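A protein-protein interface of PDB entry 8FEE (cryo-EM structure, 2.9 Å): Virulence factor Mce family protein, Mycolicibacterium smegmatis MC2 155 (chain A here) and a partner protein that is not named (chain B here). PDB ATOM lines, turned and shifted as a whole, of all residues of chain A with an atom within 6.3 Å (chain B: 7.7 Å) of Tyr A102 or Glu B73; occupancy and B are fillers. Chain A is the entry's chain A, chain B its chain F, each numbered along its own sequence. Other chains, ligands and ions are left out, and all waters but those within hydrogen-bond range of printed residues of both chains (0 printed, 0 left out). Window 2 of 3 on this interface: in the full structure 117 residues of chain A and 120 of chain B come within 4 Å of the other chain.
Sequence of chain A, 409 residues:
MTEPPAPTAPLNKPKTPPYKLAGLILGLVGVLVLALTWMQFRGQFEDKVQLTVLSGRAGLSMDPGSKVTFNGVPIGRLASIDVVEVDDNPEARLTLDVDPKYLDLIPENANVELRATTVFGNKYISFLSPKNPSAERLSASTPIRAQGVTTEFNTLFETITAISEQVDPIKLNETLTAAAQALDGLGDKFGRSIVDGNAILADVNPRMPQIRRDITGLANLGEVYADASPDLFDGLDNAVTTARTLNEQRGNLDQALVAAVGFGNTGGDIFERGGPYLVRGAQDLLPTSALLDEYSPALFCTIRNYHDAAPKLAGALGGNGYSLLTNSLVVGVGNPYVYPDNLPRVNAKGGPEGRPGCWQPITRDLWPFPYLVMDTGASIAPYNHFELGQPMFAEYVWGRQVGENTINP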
ATOM      1  N   PHE A  70     -12.657   2.365   5.938  1.00  0.00           N
ATOM      2  CA  PHE A  70     -11.644   3.290   5.454  1.00  0.00           C
ATOM      3  C   PHE A  70     -10.283   2.661   5.701  1.00  0.00           C
ATOM      4  O   PHE A  70      -9.998   2.218   6.819  1.00  0.00           O
ATOM      5  CB  PHE A  70     -11.741   4.653   6.144  1.00  0.00           C
ATOM      6  CG  PHE A  70     -10.714   5.644   5.671  1.00  0.00           C
ATOM      7  CD1 PHE A  70     -10.834   6.249   4.432  1.00  0.00           C
ATOM      8  CD2 PHE A  70      -9.629   5.973   6.466  1.00  0.00           C
ATOM      9  CE1 PHE A  70      -9.892   7.157   3.995  1.00  0.00           C
ATOM     10  CE2 PHE A  70      -8.685   6.881   6.033  1.00  0.00           C
ATOM     11  CZ  PHE A  70      -8.818   7.474   4.796  1.00  0.00           C
ATOM     12  N   VAL A  73     -10.239  -0.601   7.596  1.00  0.00           N
ATOM     13  CA  VAL A  73     -10.744  -0.680   8.964  1.00  0.00           C
ATOM     14  C   VAL A  73     -12.199  -0.230   8.974  1.00  0.00           C
ATOM     15  O   VAL A  73     -12.519   0.810   8.380  1.00  0.00           O
ATOM     16  CB  VAL A  73      -9.907   0.168   9.932  1.00  0.00           C
ATOM     17  CG1 VAL A  73     -10.269  -0.170  11.368  1.00  0.00           C
ATOM     18  CG2 VAL A  73      -8.427  -0.035   9.685  1.00  0.00           C
ATOM     19  N   PRO A  74     -13.110  -0.985   9.590  1.00  0.00           N
ATOM     20  CA  PRO A  74     -14.511  -0.551   9.638  1.00  0.00           C
ATOM     21  C   PRO A  74     -14.657   0.766  10.387  1.00  0.00           C
ATOM     22  O   PRO A  74     -14.012   0.997  11.412  1.00  0.00           O
ATOM     23  CB  PRO A  74     -15.211  -1.700  10.372  1.00  0.00           C
ATOM     24  CG  PRO A  74     -14.320  -2.876  10.166  1.00  0.00           C
ATOM     25  CD  PRO A  74     -12.930  -2.329  10.161  1.00  0.00           C
ATOM     26  N   ILE A  75     -15.520   1.630   9.859  1.00  0.00           N
ATOM     27  CA  ILE A  75     -15.762   2.956  10.413  1.00  0.00           C
ATOM     28  C   ILE A  75     -17.263   3.163  10.540  1.00  0.00           C
ATOM     29  O   ILE A  75     -17.720   4.146  11.133  1.00  0.00           O
ATOM     30  CB  ILE A  75     -15.141   4.054   9.531  1.00  0.00           C
ATOM     31  CG1 ILE A  75     -15.893   4.130   8.203  1.00  0.00           C
ATOM     32  CG2 ILE A  75     -13.654   3.820   9.313  1.00  0.00           C
ATOM     33  CD1 ILE A  75     -15.349   5.142   7.254  1.00  0.00           C
ATOM     34  N   GLY A  76     -18.034   2.244   9.981  1.00  0.00           N
ATOM     35  CA  GLY A  76     -19.474   2.382   9.999  1.00  0.00           C
ATOM     36  C   GLY A  76     -20.133   1.171   9.388  1.00  0.00           C
ATOM     37  O   GLY A  76     -19.516   0.115   9.245  1.00  0.00           O
ATOM     38  N   VAL A  98     -22.142   6.417   9.465  1.00  0.00           N
ATOM     39  CA  VAL A  98     -20.731   6.358   9.829  1.00  0.00           C
ATOM     40  C   VAL A  98     -20.508   7.181  11.091  1.00  0.00           C
ATOM     41  O   VAL A  98     -21.097   8.256  11.259  1.00  0.00           O
ATOM     42  CB  VAL A  98     -19.833   6.848   8.670  1.00  0.00           C
ATOM     43  CG1 VAL A  98     -20.341   8.158   8.127  1.00  0.00           C
ATOM     44  CG2 VAL A  98     -18.378   6.969   9.100  1.00  0.00           C
ATOM     45  N   ASP A  99     -19.686   6.648  11.992  1.00  0.00           N
ATOM     46  CA  ASP A  99     -19.313   7.361  13.208  1.00  0.00           C
ATOM     47  C   ASP A  99     -18.491   8.596  12.848  1.00  0.00           C
ATOM     48  O   ASP A  99     -17.478   8.478  12.149  1.00  0.00           O
ATOM     49  CB  ASP A  99     -18.516   6.428  14.124  1.00  0.00           C
ATOM     50  CG  ASP A  99     -18.405   6.941  15.552  1.00  0.00           C
ATOM     51  OD1 ASP A  99     -18.270   8.163  15.762  1.00  0.00           O
ATOM     52  OD2 ASP A  99     -18.450   6.105  16.478  1.00  0.00           O
ATOM     53  N   PRO A 100     -18.889   9.793  13.302  1.00  0.00           N
ATOM     54  CA  PRO A 100     -18.193  11.021  12.884  1.00  0.00           C
ATOM     55  C   PRO A 100     -16.810  11.215  13.490  1.00  0.00           C
ATOM     56  O   PRO A 100     -16.210  12.280  13.316  1.00  0.00           O
ATOM     57  CB  PRO A 100     -19.150  12.132  13.337  1.00  0.00           C
ATOM     58  CG  PRO A 100     -19.964  11.521  14.419  1.00  0.00           C
ATOM     59  CD  PRO A 100     -20.125  10.082  14.049  1.00  0.00           C
ATOM     60  N   LYS A 101     -16.291  10.216  14.208  1.00  0.00           N
ATOM     61  CA  LYS A 101     -14.904  10.283  14.662  1.00  0.00           C
ATOM     62  C   LYS A 101     -13.933  10.264  13.490  1.00  0.00           C
ATOM     63  O   LYS A 101     -12.937  10.998  13.489  1.00  0.00           O
ATOM     64  CB  LYS A 101     -14.595   9.128  15.614  1.00  0.00           C
ATOM     65  CG  LYS A 101     -15.403   9.120  16.893  1.00  0.00           C
ATOM     66  CD  LYS A 101     -14.915   8.028  17.831  1.00  0.00           C
ATOM     67  CE  LYS A 101     -14.819   6.687  17.120  1.00  0.00           C
ATOM     68  NZ  LYS A 101     -14.308   5.615  18.016  1.00  0.00           N
ATOM     69  N   TYR A 102     -14.198   9.433  12.487  1.00  0.00           N
ATOM     70  CA  TYR A 102     -13.278   9.222  11.378  1.00  0.00           C
ATOM     71  C   TYR A 102     -13.528  10.153  10.201  1.00  0.00           C
ATOM     72  O   TYR A 102     -12.764  10.114   9.231  1.00  0.00           O
ATOM     73  CB  TYR A 102     -13.359   7.770  10.903  1.00  0.00           C
ATOM     74  CG  TYR A 102     -13.338   6.761  12.025  1.00  0.00           C
ATOM     75  CD1 TYR A 102     -12.164   6.480  12.707  1.00  0.00           C
ATOM     76  CD2 TYR A 102     -14.491   6.088  12.402  1.00  0.00           C
ATOM     77  CE1 TYR A 102     -12.138   5.559  13.731  1.00  0.00           C
ATOM     78  CE2 TYR A 102     -14.475   5.163  13.425  1.00  0.00           C
ATOM     79  CZ  TYR A 102     -13.295   4.903  14.085  1.00  0.00           C
ATOM     80  OH  TYR A 102     -13.273   3.981  15.106  1.00  0.00           O
ATOM     81  N   LEU A 103     -14.581  10.975  10.251  1.00  0.00           N
ATOM     82  CA  LEU A 103     -14.848  11.906   9.158  1.00  0.00           C
ATOM     83  C   LEU A 103     -13.718  12.914   8.996  1.00  0.00           C
ATOM     84  O   LEU A 103     -13.388  13.311   7.873  1.00  0.00           O
ATOM     85  CB  LEU A 103     -16.174  12.626   9.392  1.00  0.00           C
ATOM     86  CG  LEU A 103     -17.303  12.293   8.418  1.00  0.00           C
ATOM     87  CD1 LEU A 103     -17.636  10.814   8.467  1.00  0.00           C
ATOM     88  CD2 LEU A 103     -18.528  13.136   8.719  1.00  0.00           C
ATOM     89  N   ASP A 104     -13.115  13.344  10.107  1.00  0.00           N
ATOM     90  CA  ASP A 104     -11.969  14.243  10.044  1.00  0.00           C
ATOM     91  C   ASP A 104     -10.756  13.591   9.389  1.00  0.00           C
ATOM     92  O   ASP A 104      -9.850  14.300   8.935  1.00  0.00           O
ATOM     93  CB  ASP A 104     -11.614  14.724  11.453  1.00  0.00           C
ATOM     94  CG  ASP A 104     -10.492  15.745  11.463  1.00  0.00           C
ATOM     95  OD1 ASP A 104     -10.734  16.901  11.055  1.00  0.00           O
ATOM     96  OD2 ASP A 104      -9.368  15.391  11.875  1.00  0.00           O
ATOM     97  N   LEU A 105     -10.726  12.262   9.309  1.00  0.00           N
ATOM     98  CA  LEU A 105      -9.592  11.554   8.731  1.00  0.00           C
ATOM     99  C   LEU A 105      -9.756  11.286   7.241  1.00  0.00           C
ATOM    100  O   LEU A 105      -8.754  11.214   6.518  1.00  0.00           O
ATOM    101  CB  LEU A 105      -9.383  10.230   9.468  1.00  0.00           C
ATOM    102  CG  LEU A 105      -8.048   9.507   9.304  1.00  0.00           C
ATOM    103  CD1 LEU A 105      -6.899  10.393   9.748  1.00  0.00           C
ATOM    104  CD2 LEU A 105      -8.068   8.214  10.094  1.00  0.00           C
ATOM    105  N   ILE A 106     -10.987  11.141   6.767  1.00  0.00           N
ATOM    106  CA  ILE A 106     -11.264  10.835   5.365  1.00  0.00           C
ATOM    107  C   ILE A 106     -11.236  12.111   4.532  1.00  0.00           C
ATOM    108  O   ILE A 106     -12.006  13.042   4.807  1.00  0.00           O
ATOM    109  CB  ILE A 106     -12.616  10.128   5.206  1.00  0.00           C
ATOM    110  CG1 ILE A 106     -12.670   8.878   6.075  1.00  0.00           C
ATOM    111  CG2 ILE A 106     -12.813   9.719   3.766  1.00  0.00           C
ATOM    112  CD1 ILE A 106     -14.003   8.201   6.029  1.00  0.00           C
ATOM    113  N   ALA B  45       2.432  -1.552  14.855  1.00  0.00           N
ATOM    114  CA  ALA B  45       2.736  -1.776  13.451  1.00  0.00           C
ATOM    115  C   ALA B  45       1.921  -0.817  12.597  1.00  0.00           C
ATOM    116  O   ALA B  45       0.806  -0.430  12.960  1.00  0.00           O
ATOM    117  CB  ALA B  45       2.458  -3.225  13.037  1.00  0.00           C
ATOM    118  N   LEU B  47       0.342  -0.214   8.721  1.00  0.00           N
ATOM    119  CA  LEU B  47      -0.059  -0.951   7.541  1.00  0.00           C
ATOM    120  C   LEU B  47      -0.515   0.004   6.446  1.00  0.00           C
ATOM    121  O   LEU B  47      -1.190   0.998   6.737  1.00  0.00           O
ATOM    122  CB  LEU B  47      -1.200  -1.926   7.858  1.00  0.00           C
ATOM    123  CG  LEU B  47      -1.087  -2.877   9.049  1.00  0.00           C
ATOM    124  CD1 LEU B  47      -2.373  -3.676   9.179  1.00  0.00           C
ATOM    125  CD2 LEU B  47       0.104  -3.804   8.907  1.00  0.00           C
ATOM    126  N   SER B  50      -5.594  -2.143   6.083  1.00  0.00           N
ATOM    127  CA  SER B  50      -5.873  -3.078   7.169  1.00  0.00           C
ATOM    128  C   SER B  50      -5.771  -4.521   6.701  1.00  0.00           C
ATOM    129  O   SER B  50      -5.196  -5.368   7.396  1.00  0.00           O
ATOM    130  CB  SER B  50      -7.256  -2.810   7.753  1.00  0.00           C
ATOM    131  OG  SER B  50      -7.567  -3.743   8.771  1.00  0.00           O
ATOM    132  N   LEU B  53      -7.694  -7.126   9.106  1.00  0.00           N
ATOM    133  CA  LEU B  53      -7.261  -7.455  10.456  1.00  0.00           C
ATOM    134  C   LEU B  53      -8.164  -6.782  11.482  1.00  0.00           C
ATOM    135  O   LEU B  53      -8.579  -5.633  11.311  1.00  0.00           O
ATOM    136  CB  LEU B  53      -5.811  -7.020  10.660  1.00  0.00           C
ATOM    137  CG  LEU B  53      -5.074  -7.605  11.863  1.00  0.00           C
ATOM    138  CD1 LEU B  53      -5.094  -9.117  11.801  1.00  0.00           C
ATOM    139  CD2 LEU B  53      -3.647  -7.094  11.915  1.00  0.00           C
ATOM    140  N   SER B  71      -5.717  -3.731  19.178  1.00  0.00           N
ATOM    141  CA  SER B  71      -6.553  -2.749  18.501  1.00  0.00           C
ATOM    142  C   SER B  71      -6.042  -2.512  17.087  1.00  0.00           C
ATOM    143  O   SER B  71      -4.839  -2.573  16.829  1.00  0.00           O
ATOM    144  CB  SER B  71      -6.591  -1.422  19.267  1.00  0.00           C
ATOM    145  OG  SER B  71      -5.333  -0.770  19.217  1.00  0.00           O
ATOM    146  N   VAL B  72      -6.974  -2.248  16.175  1.00  0.00           N
ATOM    147  CA  VAL B  72      -6.665  -1.839  14.809  1.00  0.00           C
ATOM    148  C   VAL B  72      -7.495  -0.602  14.501  1.00  0.00           C
ATOM    149  O   VAL B  72      -8.730  -0.654  14.550  1.00  0.00           O
ATOM    150  CB  VAL B  72      -6.953  -2.949  13.783  1.00  0.00           C
ATOM    151  CG1 VAL B  72      -6.647  -2.463  12.379  1.00  0.00           C
ATOM    152  CG2 VAL B  72      -6.144  -4.195  14.096  1.00  0.00           C
ATOM    153  N   GLU B  73      -6.825   0.507  14.183  1.00  0.00           N
ATOM    154  CA  GLU B  73      -7.514   1.779  14.034  1.00  0.00           C
ATOM    155  C   GLU B  73      -7.047   2.475  12.763  1.00  0.00           C
ATOM    156  O   GLU B  73      -5.853   2.457  12.456  1.00  0.00           O
ATOM    157  CB  GLU B  73      -7.245   2.675  15.254  1.00  0.00           C
ATOM    158  CG  GLU B  73      -8.346   3.670  15.567  1.00  0.00           C
ATOM    159  CD  GLU B  73      -9.635   2.989  15.981  1.00  0.00           C
ATOM    160  OE1 GLU B  73      -9.564   1.975  16.708  1.00  0.00           O
ATOM    161  OE2 GLU B  73     -10.718   3.462  15.580  1.00  0.00           O
ATOM    162  N   PRO B  74      -7.950   3.094  12.004  1.00  0.00           N
ATOM    163  CA  PRO B  74      -7.521   3.798  10.791  1.00  0.00           C
ATOM    164  C   PRO B  74      -6.636   4.992  11.111  1.00  0.00           C
ATOM    165  O   PRO B  74      -6.757   5.624  12.162  1.00  0.00           O
ATOM    166  CB  PRO B  74      -8.840   4.240  10.148  1.00  0.00           C
ATOM    167  CG  PRO B  74      -9.809   4.276  11.262  1.00  0.00           C
ATOM    168  CD  PRO B  74      -9.405   3.186  12.205  1.00  0.00           C
ATOM    169  N   SER B  75      -5.729   5.292  10.182  1.00  0.00           N
ATOM    170  CA  SER B  75      -4.831   6.428  10.334  1.00  0.00           C
ATOM    171  C   SER B  75      -4.810   7.255   9.056  1.00  0.00           C
ATOM    172  O   SER B  75      -5.609   7.016   8.144  1.00  0.00           O
ATOM    173  CB  SER B  75      -3.420   5.961  10.693  1.00  0.00           C
ATOM    174  OG  SER B  75      -2.825   5.261   9.618  1.00  0.00           O
ATOM    175  N   GLU B  76      -3.908   8.232   8.980  1.00  0.00           N
ATOM    176  CA  GLU B  76      -3.784   9.032   7.767  1.00  0.00           C
ATOM    177  C   GLU B  76      -3.035   8.294   6.664  1.00  0.00           C
ATOM    178  O   GLU B  76      -3.348   8.477   5.482  1.00  0.00           O
ATOM    179  CB  GLU B  76      -3.094  10.365   8.072  1.00  0.00           C
ATOM    180  CG  GLU B  76      -1.740  10.258   8.767  1.00  0.00           C
ATOM    181  CD  GLU B  76      -1.853  10.094  10.271  1.00  0.00           C
ATOM    182  OE1 GLU B  76      -2.984  10.174  10.795  1.00  0.00           O
ATOM    183  OE2 GLU B  76      -0.812   9.882  10.928  1.00  0.00           O
ATOM    184  N   GLY B  78      -2.728   4.865   6.488  1.00  0.00           N
ATOM    185  CA  GLY B  78      -3.096   3.464   6.480  1.00  0.00           C
ATOM    186  C   GLY B  78      -3.828   3.044   7.737  1.00  0.00           C
ATOM    187  O   GLY B  78      -4.850   3.640   8.089  1.00  0.00           O
ATOM    188  N   ALA B  79      -3.323   2.022   8.421  1.00  0.00           N
ATOM    189  CA  ALA B  79      -3.909   1.563   9.670  1.00  0.00           C
ATOM    190  C   ALA B  79      -2.821   1.357  10.713  1.00  0.00           C
ATOM    191  O   ALA B  79      -1.692   0.977  10.394  1.00  0.00           O
ATOM    192  CB  ALA B  79      -4.697   0.264   9.476  1.00  0.00           C
ATOM    193  N   ARG B  80      -3.170   1.623  11.966  1.00  0.00           N
ATOM    194  CA  ARG B  80      -2.274   1.464  13.100  1.00  0.00           C
ATOM    195  C   ARG B  80      -2.740   0.271  13.921  1.00  0.00           C
ATOM    196  O   ARG B  80      -3.917   0.190  14.290  1.00  0.00           O
ATOM    197  CB  ARG B  80      -2.253   2.731  13.957  1.00  0.00           C
ATOM    198  CG  ARG B  80      -1.274   2.695  15.115  1.00  0.00           C
ATOM    199  CD  ARG B  80       0.152   2.589  14.612  1.00  0.00           C
ATOM    200  NE  ARG B  80       1.119   2.543  15.702  1.00  0.00           N
ATOM    201  CZ  ARG B  80       1.696   3.612  16.233  1.00  0.00           C
ATOM    202  NH1 ARG B  80       1.423   4.831  15.800  1.00  0.00           N
ATOM    203  NH2 ARG B  80       2.570   3.453  17.222  1.00  0.00           N
ATOM    204  N   VAL B  81      -1.823  -0.650  14.199  1.00  0.00           N
ATOM    205  CA  VAL B  81      -2.136  -1.894  14.888  1.00  0.00           C
ATOM    206  C   VAL B  81      -1.342  -1.935  16.183  1.00  0.00           C
ATOM    207  O   VAL B  81      -0.116  -1.792  16.167  1.00  0.00           O
ATOM    208  CB  VAL B  81      -1.824  -3.122  14.012  1.00  0.00           C
ATOM    209  CG1 VAL B  81      -2.026  -4.400  14.799  1.00  0.00           C
ATOM    210  CG2 VAL B  81      -2.700  -3.117  12.777  1.00  0.00           C
ATOM    211  N   GLU B  82      -2.040  -2.122  17.297  1.00  0.00           N
ATOM    212  CA  GLU B  82      -1.421  -2.290  18.602  1.00  0.00           C
ATOM    213  C   GLU B  82      -1.685  -3.710  19.076  1.00  0.00           C
ATOM    214  O   GLU B  82      -2.828  -4.180  19.026  1.00  0.00           O
ATOM    215  CB  GLU B  82      -1.974  -1.280  19.609  1.00  0.00           C
ATOM    216  CG  GLU B  82      -1.597   0.160  19.314  1.00  0.00           C
ATOM    217  CD  GLU B  82      -2.136   1.124  20.349  1.00  0.00           C
ATOM    218  OE1 GLU B  82      -3.032   0.727  21.121  1.00  0.00           O
ATOM    219  OE2 GLU B  82      -1.665   2.279  20.390  1.00  0.00           O
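OE2 of Glu B73 sits at hydrogen-bond distance from OH of Tyr A102 (2.6 Å).
The backbone carbonyl oxygen (O) of Ala B79 lies within hydrogen-bond range of the backbone NH (N) of Leu B47 (2.9 Å).
The backbone NH (N) of Ala B79 lies within hydrogen-bond range of the side-chain hydroxyl (OG) of Ser B75 (3.5 Å).
OG of Ser B75 sits at hydrogen-bond distance from O of Gly B78 (3.0 Å).
The side-chain hydroxyl of Tyr A102 lies within hydrogen-bond range of the side-chain amino group of Lys A101, 3.5 Å away.
The backbone NH of Arg B80 sits at hydrogen-bond distance from the backbone carbonyl oxygen of Glu B73.
The side-chain hydroxyl (OG) of Ser B50 lies within hydrogen-bond range of the backbone carbonyl oxygen (O) of Leu B53, 3.3 Å away.
Phe A70 touches Ser B75 (CE2 to O, 3.7 Å).
Val A73 touches Ser B50.
Val B72 touches Val A73 (O to CG1, 3.6 Å).
Val A73 touches Pro B74.
Ala B79 touches Val A73 (CB to CG2, 3.7 Å).
Pro B74 touches Tyr A102.
CD2 of Leu A105 touches O of Pro B74, 3.6 Å away.
Leu A105 touches Ser B75 (CD2 to O, 3.4 Å).
N of Glu B76 touches CD1 of Leu A105, at 3.8 Å.
Printed residues of chain B within 4 Å of Val A73: Ser B50, Val B72, Pro B74 and Ala B79.
Tyr A102 touches just these residues of chain B: Glu B73 and Pro B74.
Of the printed residues of chain A, Val B72 touches Val A73 (3.6 Å).
Of chain A, only Tyr A102 (2.6 Å) comes within 4 Å of Glu B73.
Printed residues of chain A within 4 Å of Pro B74: Val A73 (3.6 Å), Tyr A102 (3.5 Å) and Leu A105 (3.6 Å).
Printed residues of chain A within 4 Å of Glu B76: Leu A105.
Printed residues of chain A within 4 Å of Ala B79: Val A73 (3.7 Å).
The nearest residue of chain A that does not touch Glu B73 is Val A73 (4.2 Å).
The nearest printed residue of chain B that does not touch Phe A70 is Pro B74 (4.1 Å).
Of the 14 printed residues of chain A, 4 touch a printed residue of chain B.
Printed residues of chain A that touch a printed residue of chain B: Phe A70, Val A73, Tyr A102 and Leu A105.
Hydrophobic or aromatic side chains of chain A within 4 Å of the printed part of chain B: Phe A70, Val A73, Tyr A102 and Leu A105.
Printed residues of chain B that touch a printed residue of chain A: Ser B50, Val B72, Glu B73, Pro B74, Ser B75, Glu B76 and Ala B79.
Hydrophobic or aromatic side chains of chain B within 4 Å of the printed part of chain A: Pro B74 and Ala B79.
Among the printed residues, no Asp or Glu carboxylate lies within 4 Å of a Lys or Arg side-chain nitrogen of the other chain.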
